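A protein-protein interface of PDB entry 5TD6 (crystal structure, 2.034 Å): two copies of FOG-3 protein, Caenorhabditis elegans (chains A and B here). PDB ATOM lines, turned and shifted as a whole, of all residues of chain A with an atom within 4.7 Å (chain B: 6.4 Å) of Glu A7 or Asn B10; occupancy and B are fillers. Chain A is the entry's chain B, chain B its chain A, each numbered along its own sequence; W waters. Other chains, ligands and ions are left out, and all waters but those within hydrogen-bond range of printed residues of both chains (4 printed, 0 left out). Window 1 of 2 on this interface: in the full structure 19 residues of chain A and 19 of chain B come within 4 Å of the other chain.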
ATOM      1  N   THR A   3      30.659  17.433 -18.990  1.00  0.00           N
ATOM      2  CA  THR A   3      29.971  16.788 -17.861  1.00  0.00           C
ATOM      3  C   THR A   3      30.990  16.208 -16.874  1.00  0.00           C
ATOM      4  O   THR A   3      30.941  16.490 -15.669  1.00  0.00           O
ATOM      5  CB  THR A   3      29.056  15.653 -18.349  1.00  0.00           C
ATOM      6  OG1 THR A   3      28.103  16.170 -19.282  1.00  0.00           O
ATOM      7  CG2 THR A   3      28.324  14.955 -17.185  1.00  0.00           C
ATOM      8  N   GLU A   4      31.916  15.397 -17.391  1.00  0.00           N
ATOM      9  CA  GLU A   4      32.877  14.719 -16.522  1.00  0.00           C
ATOM     10  C   GLU A   4      33.784  15.720 -15.809  1.00  0.00           C
ATOM     11  O   GLU A   4      34.043  15.594 -14.610  1.00  0.00           O
ATOM     12  CB  GLU A   4      33.716  13.713 -17.320  1.00  0.00           C
ATOM     13  CG  GLU A   4      32.948  12.503 -17.824  1.00  0.00           C
ATOM     14  CD  GLU A   4      32.263  12.744 -19.188  1.00  0.00           C
ATOM     15  OE1 GLU A   4      32.236  13.893 -19.699  1.00  0.00           O
ATOM     16  OE2 GLU A   4      31.741  11.769 -19.741  1.00  0.00           O
ATOM     17  N   VAL A   5      34.257  16.723 -16.541  1.00  0.00           N
ATOM     18  CA  VAL A   5      35.093  17.766 -15.950  1.00  0.00           C
ATOM     19  C   VAL A   5      34.322  18.499 -14.868  1.00  0.00           C
ATOM     20  O   VAL A   5      34.847  18.790 -13.814  1.00  0.00           O
ATOM     21  CB  VAL A   5      35.572  18.800 -17.002  1.00  0.00           C
ATOM     22  CG1 VAL A   5      36.170  19.987 -16.319  1.00  0.00           C
ATOM     23  CG2 VAL A   5      36.581  18.168 -17.977  1.00  0.00           C
ATOM     24  N   ARG A   6      33.058  18.797 -15.140  1.00  0.00           N
ATOM     25  CA  ARG A   6      32.265  19.508 -14.152  1.00  0.00           C
ATOM     26  C   ARG A   6      32.096  18.665 -12.897  1.00  0.00           C
ATOM     27  O   ARG A   6      32.162  19.199 -11.787  1.00  0.00           O
ATOM     28  CB  ARG A   6      30.885  19.890 -14.703  1.00  0.00           C
ATOM     29  CG  ARG A   6      30.032  20.652 -13.687  1.00  0.00           C
ATOM     30  CD  ARG A   6      28.631  20.934 -14.228  1.00  0.00           C
ATOM     31  NE  ARG A   6      27.861  19.706 -14.401  1.00  0.00           N
ATOM     32  CZ  ARG A   6      27.420  19.258 -15.575  1.00  0.00           C
ATOM     33  NH1 ARG A   6      27.675  19.934 -16.692  1.00  0.00           N
ATOM     34  NH2 ARG A   6      26.723  18.130 -15.636  1.00  0.00           N
ATOM     35  N   GLU A   7      31.863  17.356 -13.066  1.00  0.00           N
ATOM     36  CA  GLU A   7      31.728  16.482 -11.902  1.00  0.00           C
ATOM     37  C   GLU A   7      33.045  16.408 -11.108  1.00  0.00           C
ATOM     38  O   GLU A   7      33.024  16.378  -9.873  1.00  0.00           O
ATOM     39  CB  GLU A   7      31.277  15.084 -12.316  1.00  0.00           C
ATOM     40  CG  GLU A   7      29.815  15.024 -12.828  1.00  0.00           C
ATOM     41  CD  GLU A   7      28.836  15.519 -11.801  1.00  0.00           C
ATOM     42  OE1 GLU A   7      29.004  15.177 -10.615  1.00  0.00           O
ATOM     43  OE2 GLU A   7      27.906  16.259 -12.171  1.00  0.00           O
ATOM     44  N   LEU A   8      34.175  16.365 -11.810  1.00  0.00           N
ATOM     45  CA  LEU A   8      35.494  16.345 -11.150  1.00  0.00           C
ATOM     46  C   LEU A   8      35.710  17.644 -10.378  1.00  0.00           C
ATOM     47  O   LEU A   8      36.118  17.640  -9.200  1.00  0.00           O
ATOM     48  CB  LEU A   8      36.622  16.148 -12.165  1.00  0.00           C
ATOM     49  CG  LEU A   8      37.908  15.460 -11.660  1.00  0.00           C
ATOM     50  CD1 LEU A   8      38.884  15.094 -12.781  1.00  0.00           C
ATOM     51  CD2 LEU A   8      38.616  16.265 -10.631  1.00  0.00           C
ATOM     52  N   VAL A   9      35.451  18.761 -11.049  1.00  0.00           N
ATOM     53  CA  VAL A   9      35.646  20.072 -10.420  1.00  0.00           C
ATOM     54  C   VAL A   9      34.766  20.221  -9.190  1.00  0.00           C
ATOM     55  O   VAL A   9      35.194  20.741  -8.153  1.00  0.00           O
ATOM     56  CB  VAL A   9      35.334  21.220 -11.394  1.00  0.00           C
ATOM     57  CG1 VAL A   9      35.300  22.547 -10.650  1.00  0.00           C
ATOM     58  CG2 VAL A   9      36.373  21.252 -12.512  1.00  0.00           C
ATOM     59  N   ASN A  10      33.537  19.744  -9.294  1.00  0.00           N
ATOM     60  CA  ASN A  10      32.613  19.912  -8.177  1.00  0.00           C
ATOM     61  C   ASN A  10      32.991  18.983  -7.023  1.00  0.00           C
ATOM     62  O   ASN A  10      32.858  19.350  -5.854  1.00  0.00           O
ATOM     63  CB  ASN A  10      31.174  19.713  -8.643  1.00  0.00           C
ATOM     64  CG  ASN A  10      30.672  20.915  -9.408  1.00  0.00           C
ATOM     65  OD1 ASN A  10      31.373  21.907  -9.483  1.00  0.00           O
ATOM     66  ND2 ASN A  10      29.470  20.847  -9.952  1.00  0.00           N
ATOM     67  N   PHE A  11      33.503  17.803  -7.351  1.00  0.00           N
ATOM     68  CA  PHE A  11      34.052  16.917  -6.324  1.00  0.00           C
ATOM     69  C   PHE A  11      35.140  17.605  -5.495  1.00  0.00           C
ATOM     70  O   PHE A  11      35.128  17.556  -4.263  1.00  0.00           O
ATOM     71  CB  PHE A  11      34.628  15.646  -6.961  1.00  0.00           C
ATOM     72  CG  PHE A  11      35.209  14.675  -5.950  1.00  0.00           C
ATOM     73  CD1 PHE A  11      34.393  13.784  -5.274  1.00  0.00           C
ATOM     74  CD2 PHE A  11      36.565  14.673  -5.669  1.00  0.00           C
ATOM     75  CE1 PHE A  11      34.911  12.891  -4.365  1.00  0.00           C
ATOM     76  CE2 PHE A  11      37.090  13.777  -4.748  1.00  0.00           C
ATOM     77  CZ  PHE A  11      36.261  12.896  -4.092  1.00  0.00           C
ATOM     78  N   VAL A  97      33.719   9.108 -13.759  1.00  0.00           N
ATOM     79  CA  VAL A  97      34.633   9.853 -12.914  1.00  0.00           C
ATOM     80  C   VAL A  97      34.662   9.118 -11.585  1.00  0.00           C
ATOM     81  O   VAL A  97      33.613   8.689 -11.070  1.00  0.00           O
ATOM     82  CB  VAL A  97      34.177  11.308 -12.728  1.00  0.00           C
ATOM     83  CG1 VAL A  97      35.210  12.111 -11.919  1.00  0.00           C
ATOM     84  CG2 VAL A  97      33.949  11.949 -14.077  1.00  0.00           C
ATOM     85  N   ILE A 110      32.429   8.785  -8.517  1.00  0.00           N
ATOM     86  CA  ILE A 110      32.051  10.173  -8.345  1.00  0.00           C
ATOM     87  C   ILE A 110      30.851  10.466  -9.276  1.00  0.00           C
ATOM     88  O   ILE A 110      29.863  11.082  -8.875  1.00  0.00           O
ATOM     89  CB  ILE A 110      33.203  11.133  -8.679  1.00  0.00           C
ATOM     90  CG1 ILE A 110      34.353  10.961  -7.672  1.00  0.00           C
ATOM     91  CG2 ILE A 110      32.656  12.569  -8.711  1.00  0.00           C
ATOM     92  CD1 ILE A 110      35.673  11.671  -8.101  1.00  0.00           C
ATOM     93  N   TRP A 111      30.955  10.011 -10.515  1.00  0.00           N
ATOM     94  CA  TRP A 111      29.856  10.115 -11.476  1.00  0.00           C
ATOM     95  C   TRP A 111      29.949   9.022 -12.533  1.00  0.00           C
ATOM     96  O   TRP A 111      31.050   8.663 -12.983  1.00  0.00           O
ATOM     97  CB  TRP A 111      29.840  11.498 -12.142  1.00  0.00           C
ATOM     98  CG  TRP A 111      28.691  11.692 -13.162  1.00  0.00           C
ATOM     99  CD1 TRP A 111      27.399  12.066 -12.896  1.00  0.00           C
ATOM    100  CD2 TRP A 111      28.769  11.511 -14.584  1.00  0.00           C
ATOM    101  NE1 TRP A 111      26.671  12.138 -14.071  1.00  0.00           N
ATOM    102  CE2 TRP A 111      27.490  11.801 -15.119  1.00  0.00           C
ATOM    103  CE3 TRP A 111      29.795  11.127 -15.458  1.00  0.00           C
ATOM    104  CZ2 TRP A 111      27.216  11.722 -16.483  1.00  0.00           C
ATOM    105  CZ3 TRP A 111      29.520  11.050 -16.817  1.00  0.00           C
ATOM    106  CH2 TRP A 111      28.248  11.353 -17.317  1.00  0.00           C
ATOM    107  N   VAL B   5      19.287  22.147  -8.339  1.00  0.00           N
ATOM    108  CA  VAL B   5      18.561  20.879  -8.451  1.00  0.00           C
ATOM    109  C   VAL B   5      19.464  19.757  -8.980  1.00  0.00           C
ATOM    110  O   VAL B   5      19.454  18.630  -8.471  1.00  0.00           O
ATOM    111  CB  VAL B   5      17.316  21.030  -9.371  1.00  0.00           C
ATOM    112  CG1 VAL B   5      16.849  19.667  -9.914  1.00  0.00           C
ATOM    113  CG2 VAL B   5      16.194  21.729  -8.630  1.00  0.00           C
ATOM    114  N   ARG B   6      20.272  20.073  -9.983  1.00  0.00           N
ATOM    115  CA  ARG B   6      21.221  19.086 -10.487  1.00  0.00           C
ATOM    116  C   ARG B   6      22.193  18.579  -9.410  1.00  0.00           C
ATOM    117  O   ARG B   6      22.455  17.383  -9.319  1.00  0.00           O
ATOM    118  CB  ARG B   6      22.034  19.646 -11.654  1.00  0.00           C
ATOM    119  CG  ARG B   6      23.113  18.621 -12.100  1.00  0.00           C
ATOM    120  CD  ARG B   6      23.716  18.973 -13.424  1.00  0.00           C
ATOM    121  NE  ARG B   6      24.398  20.255 -13.385  1.00  0.00           N
ATOM    122  CZ  ARG B   6      24.652  20.958 -14.485  1.00  0.00           C
ATOM    123  NH1 ARG B   6      24.267  20.484 -15.668  1.00  0.00           N
ATOM    124  NH2 ARG B   6      25.274  22.126 -14.409  1.00  0.00           N
ATOM    125  N   GLU B   7      22.727  19.492  -8.602  1.00  0.00           N
ATOM    126  CA  GLU B   7      23.670  19.126  -7.553  1.00  0.00           C
ATOM    127  C   GLU B   7      22.988  18.281  -6.483  1.00  0.00           C
ATOM    128  O   GLU B   7      23.569  17.324  -5.955  1.00  0.00           O
ATOM    129  CB  GLU B   7      24.290  20.377  -6.928  1.00  0.00           C
ATOM    130  CG  GLU B   7      25.232  21.119  -7.864  1.00  0.00           C
ATOM    131  CD  GLU B   7      26.228  20.168  -8.554  1.00  0.00           C
ATOM    132  OE1 GLU B   7      26.976  19.437  -7.868  1.00  0.00           O
ATOM    133  OE2 GLU B   7      26.241  20.139  -9.795  1.00  0.00           O
ATOM    134  N   LEU B   8      21.750  18.625  -6.163  1.00  0.00           N
ATOM    135  CA  LEU B   8      20.969  17.795  -5.253  1.00  0.00           C
ATOM    136  C   LEU B   8      20.790  16.385  -5.825  1.00  0.00           C
ATOM    137  O   LEU B   8      21.049  15.382  -5.148  1.00  0.00           O
ATOM    138  CB  LEU B   8      19.608  18.420  -4.982  1.00  0.00           C
ATOM    139  CG  LEU B   8      18.838  17.886  -3.759  1.00  0.00           C
ATOM    140  CD1 LEU B   8      17.789  18.897  -3.329  1.00  0.00           C
ATOM    141  CD2 LEU B   8      18.152  16.551  -4.028  1.00  0.00           C
ATOM    142  N   VAL B   9      20.312  16.321  -7.062  1.00  0.00           N
ATOM    143  CA  VAL B   9      20.057  15.037  -7.712  1.00  0.00           C
ATOM    144  C   VAL B   9      21.317  14.163  -7.753  1.00  0.00           C
ATOM    145  O   VAL B   9      21.259  12.973  -7.459  1.00  0.00           O
ATOM    146  CB  VAL B   9      19.511  15.242  -9.144  1.00  0.00           C
ATOM    147  CG1 VAL B   9      19.562  13.938  -9.928  1.00  0.00           C
ATOM    148  CG2 VAL B   9      18.080  15.801  -9.087  1.00  0.00           C
ATOM    149  N   ASN B  10      22.456  14.761  -8.105  1.00  0.00           N
ATOM    150  CA  ASN B  10      23.692  13.993  -8.229  1.00  0.00           C
ATOM    151  C   ASN B  10      24.197  13.516  -6.877  1.00  0.00           C
ATOM    152  O   ASN B  10      24.783  12.427  -6.767  1.00  0.00           O
ATOM    153  CB  ASN B  10      24.764  14.816  -8.941  1.00  0.00           C
ATOM    154  CG  ASN B  10      24.421  15.044 -10.402  1.00  0.00           C
ATOM    155  OD1 ASN B  10      23.473  14.453 -10.899  1.00  0.00           O
ATOM    156  ND2 ASN B  10      25.197  15.875 -11.090  1.00  0.00           N
ATOM    157  N   PHE B  11      23.958  14.329  -5.854  1.00  0.00           N
ATOM    158  CA  PHE B  11      24.275  13.939  -4.495  1.00  0.00           C
ATOM    159  C   PHE B  11      23.566  12.629  -4.167  1.00  0.00           C
ATOM    160  O   PHE B  11      24.178  11.675  -3.681  1.00  0.00           O
ATOM    161  CB  PHE B  11      23.863  15.016  -3.482  1.00  0.00           C
ATOM    162  CG  PHE B  11      23.967  14.545  -2.041  1.00  0.00           C
ATOM    163  CD1 PHE B  11      25.200  14.496  -1.411  1.00  0.00           C
ATOM    164  CD2 PHE B  11      22.834  14.138  -1.335  1.00  0.00           C
ATOM    165  CE1 PHE B  11      25.311  14.062  -0.076  1.00  0.00           C
ATOM    166  CE2 PHE B  11      22.931  13.698  -0.006  1.00  0.00           C
ATOM    167  CZ  PHE B  11      24.187  13.662   0.619  1.00  0.00           C
ATOM    168  N   VAL B  12      22.262  12.606  -4.408  1.00  0.00           N
ATOM    169  CA  VAL B  12      21.465  11.414  -4.170  1.00  0.00           C
ATOM    170  C   VAL B  12      21.952  10.257  -5.055  1.00  0.00           C
ATOM    171  O   VAL B  12      22.134   9.128  -4.570  1.00  0.00           O
ATOM    172  CB  VAL B  12      19.969  11.670  -4.446  1.00  0.00           C
ATOM    173  CG1 VAL B  12      19.170  10.352  -4.349  1.00  0.00           C
ATOM    174  CG2 VAL B  12      19.420  12.737  -3.481  1.00  0.00           C
ATOM    175  N   CYS B  13      22.198  10.539  -6.338  1.00  0.00           N
ATOM    176  CA  CYS B  13      22.619   9.475  -7.258  1.00  0.00           C
ATOM    177  C   CYS B  13      23.984   8.894  -6.887  1.00  0.00           C
ATOM    178  O   CYS B  13      24.267   7.740  -7.187  1.00  0.00           O
ATOM    179  CB  CYS B  13      22.625   9.978  -8.709  1.00  0.00           C
ATOM    180  SG  CYS B  13      20.925  10.193  -9.396  1.00  0.00           S
ATOM    181  N   ARG B  14      24.831   9.676  -6.221  1.00  0.00           N
ATOM    182  CA  ARG B  14      26.131   9.139  -5.803  1.00  0.00           C
ATOM    183  C   ARG B  14      26.000   7.988  -4.773  1.00  0.00           C
ATOM    184  O   ARG B  14      26.927   7.201  -4.617  1.00  0.00           O
ATOM    185  CB  ARG B  14      27.042  10.249  -5.267  1.00  0.00           C
ATOM    186  CG  ARG B  14      27.661  11.093  -6.394  1.00  0.00           C
ATOM    187  CD  ARG B  14      28.758  12.078  -5.946  1.00  0.00           C
ATOM    188  NE  ARG B  14      28.326  13.193  -5.085  1.00  0.00           N
ATOM    189  CZ  ARG B  14      27.862  14.366  -5.521  1.00  0.00           C
ATOM    190  NH1 ARG B  14      27.692  14.580  -6.823  1.00  0.00           N
ATOM    191  NH2 ARG B  14      27.552  15.337  -4.653  1.00  0.00           N
ATOM    192  N   TYR B  15      24.838   7.846  -4.125  1.00  0.00           N
ATOM    193  CA  TYR B  15      24.603   6.643  -3.306  1.00  0.00           C
ATOM    194  C   TYR B  15      24.264   5.427  -4.182  1.00  0.00           C
ATOM    195  O   TYR B  15      24.308   4.278  -3.717  1.00  0.00           O
ATOM    196  CB  TYR B  15      23.473   6.870  -2.299  1.00  0.00           C
ATOM    197  CG  TYR B  15      23.861   7.772  -1.166  1.00  0.00           C
ATOM    198  CD1 TYR B  15      24.624   7.291  -0.092  1.00  0.00           C
ATOM    199  CD2 TYR B  15      23.473   9.107  -1.165  1.00  0.00           C
ATOM    200  CE1 TYR B  15      24.995   8.130   0.953  1.00  0.00           C
ATOM    201  CE2 TYR B  15      23.822   9.942  -0.141  1.00  0.00           C
ATOM    202  CZ  TYR B  15      24.581   9.458   0.914  1.00  0.00           C
ATOM    203  OH  TYR B  15      24.914  10.321   1.911  1.00  0.00           O
ATOM    204  N   PHE B  17      25.299   4.999  -7.799  1.00  0.00           N
ATOM    205  CA  PHE B  17      26.308   4.633  -8.803  1.00  0.00           C
ATOM    206  C   PHE B  17      27.064   3.408  -8.344  1.00  0.00           C
ATOM    207  O   PHE B  17      27.540   3.369  -7.205  1.00  0.00           O
ATOM    208  CB  PHE B  17      27.317   5.774  -9.048  1.00  0.00           C
ATOM    209  CG  PHE B  17      26.721   7.025  -9.680  1.00  0.00           C
ATOM    210  CD1 PHE B  17      25.759   6.941 -10.685  1.00  0.00           C
ATOM    211  CD2 PHE B  17      27.149   8.287  -9.279  1.00  0.00           C
ATOM    212  CE1 PHE B  17      25.215   8.108 -11.259  1.00  0.00           C
ATOM    213  CE2 PHE B  17      26.616   9.448  -9.847  1.00  0.00           C
ATOM    214  CZ  PHE B  17      25.650   9.352 -10.840  1.00  0.00           C
HETATM  215  O   HOH W   1      25.963  16.074 -14.080  1.00  0.00           O
HETATM  216  O   HOH W   2      27.474  18.664 -11.696  1.00  0.00           O
HETATM  217  O   HOH W   3      27.938  13.012  -9.363  1.00  0.00           O
HETATM  218  O   HOH W   4      27.472  16.676  -8.914  1.00  0.00           O
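The side-chain amide nitrogen (ND2) of Asn B10 sits at hydrogen-bond distance from the side-chain carboxylate (OE2) of Glu A7 (2.9 Å). The guanidinium group (NH2) of Arg A6 lies close to the guanidinium group (NH1) of Arg B6, at 3.4 Å. The side-chain amide nitrogen (ND2) of Asn A10 lies within hydrogen-bond range of the side-chain carboxylate (OE2) of Glu B7, at 3.3 Å.
The backbone carbonyl oxygen of Trp A111 lies within hydrogen-bond range of the backbone NH of Val A97, 2.8 Å away. O of Val A97 is in hydrogen-bond range of N of Ile A110, at 2.8 Å. The backbone carbonyl oxygen of Arg B6 lies close to the side-chain amide oxygen of Asn B10 (3.5 Å).
Ile A110 touches Arg B14 (O to CD, 3.3 Å). Phe B17 touches Ile A110. Trp A111 touches Phe B17 (CA to CE2, 3.7 Å).
Val A5 touches none of the printed residues of chain B. Glu A7 touches just one residue of chain B: Asn B10 (2.9 Å). Leu A8 touches none of the printed residues of chain B. Printed residues of chain B within 4 Å of Asn A10: Glu B7. Printed residues of chain B within 4 Å of Ile A110: Arg B14 (3.3 Å) and Phe B17 (3.8 Å). Of the printed residues of chain A, Glu B7 touches Asn A10 (3.3 Å). Of chain A, only Glu A7 comes within 4 Å of Asn B10. Printed residues of chain A within 4 Å of Arg B14: Ile A110 (3.3 Å). Of the printed residues of chain A, Phe B17 touches Ile A110 and Trp A111. The nearest printed residue of chain A that does not touch Asn B10 is Trp A111 (4.8 Å). The nearest printed residue of chain A that does not touch Arg B6 is Glu A7 (5.1 Å).
Of the 12 printed residues of chain B, 5 touch a printed residue of chain A. Hydrophobic or aromatic side chains of chain B that line the printed part of chain A: Phe B17. Of the 12 printed residues of chain A, 5 touch a printed residue of chain B. Printed residues of chain A that touch a printed residue of chain B: Arg A6, Glu A7, Asn A10, Ile A110 and Trp A111. Hydrophobic or aromatic side chains of chain A that line the printed part of chain B: Trp A111. Among the printed residues, no Asp or Glu carboxylate lies within 4 Å of a Lys or Arg side-chain nitrogen of the other chain.
Arg A6 touches its own counterpart, Arg B6. Glu A7 touches Asn B10, and with the chains exchanged Asn A10 touches Glu B7. Positions printed for both chains: 5, 6, 7, 8, 9, 10 and 11. Of the 6 pairs that touch across the chains among the printed residues, 3 have their exchanged pair printed and touching as well.
Water W2 lies within hydrogen-bond range of OE2 of Glu A7 (2.5 Å), OE2 of Glu B7 (2.7 Å), NE of Arg A6 (2.9 Å) and ND2 of Asn A10 (3.4 Å). Water W1 lies within hydrogen-bond range of the guanidinium group of Arg A6, the side-chain carboxylate of Glu A7 and the side-chain amide nitrogen of Asn B10. Water W3 lies within hydrogen-bond range of OE1 of Glu A7, O of Ile A110 and NH1 of Arg B14. Water W4 lies within hydrogen-bond range of the side-chain carboxylate (OE1) of Glu A7 (2.7 Å), the guanidinium group (NH1) of Arg B14 (3.0 Å), the side-chain carboxylate (OE1) of Glu B7 (3.0 Å) and the side-chain amide nitrogen (ND2) of Asn B10 (3.2 Å).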
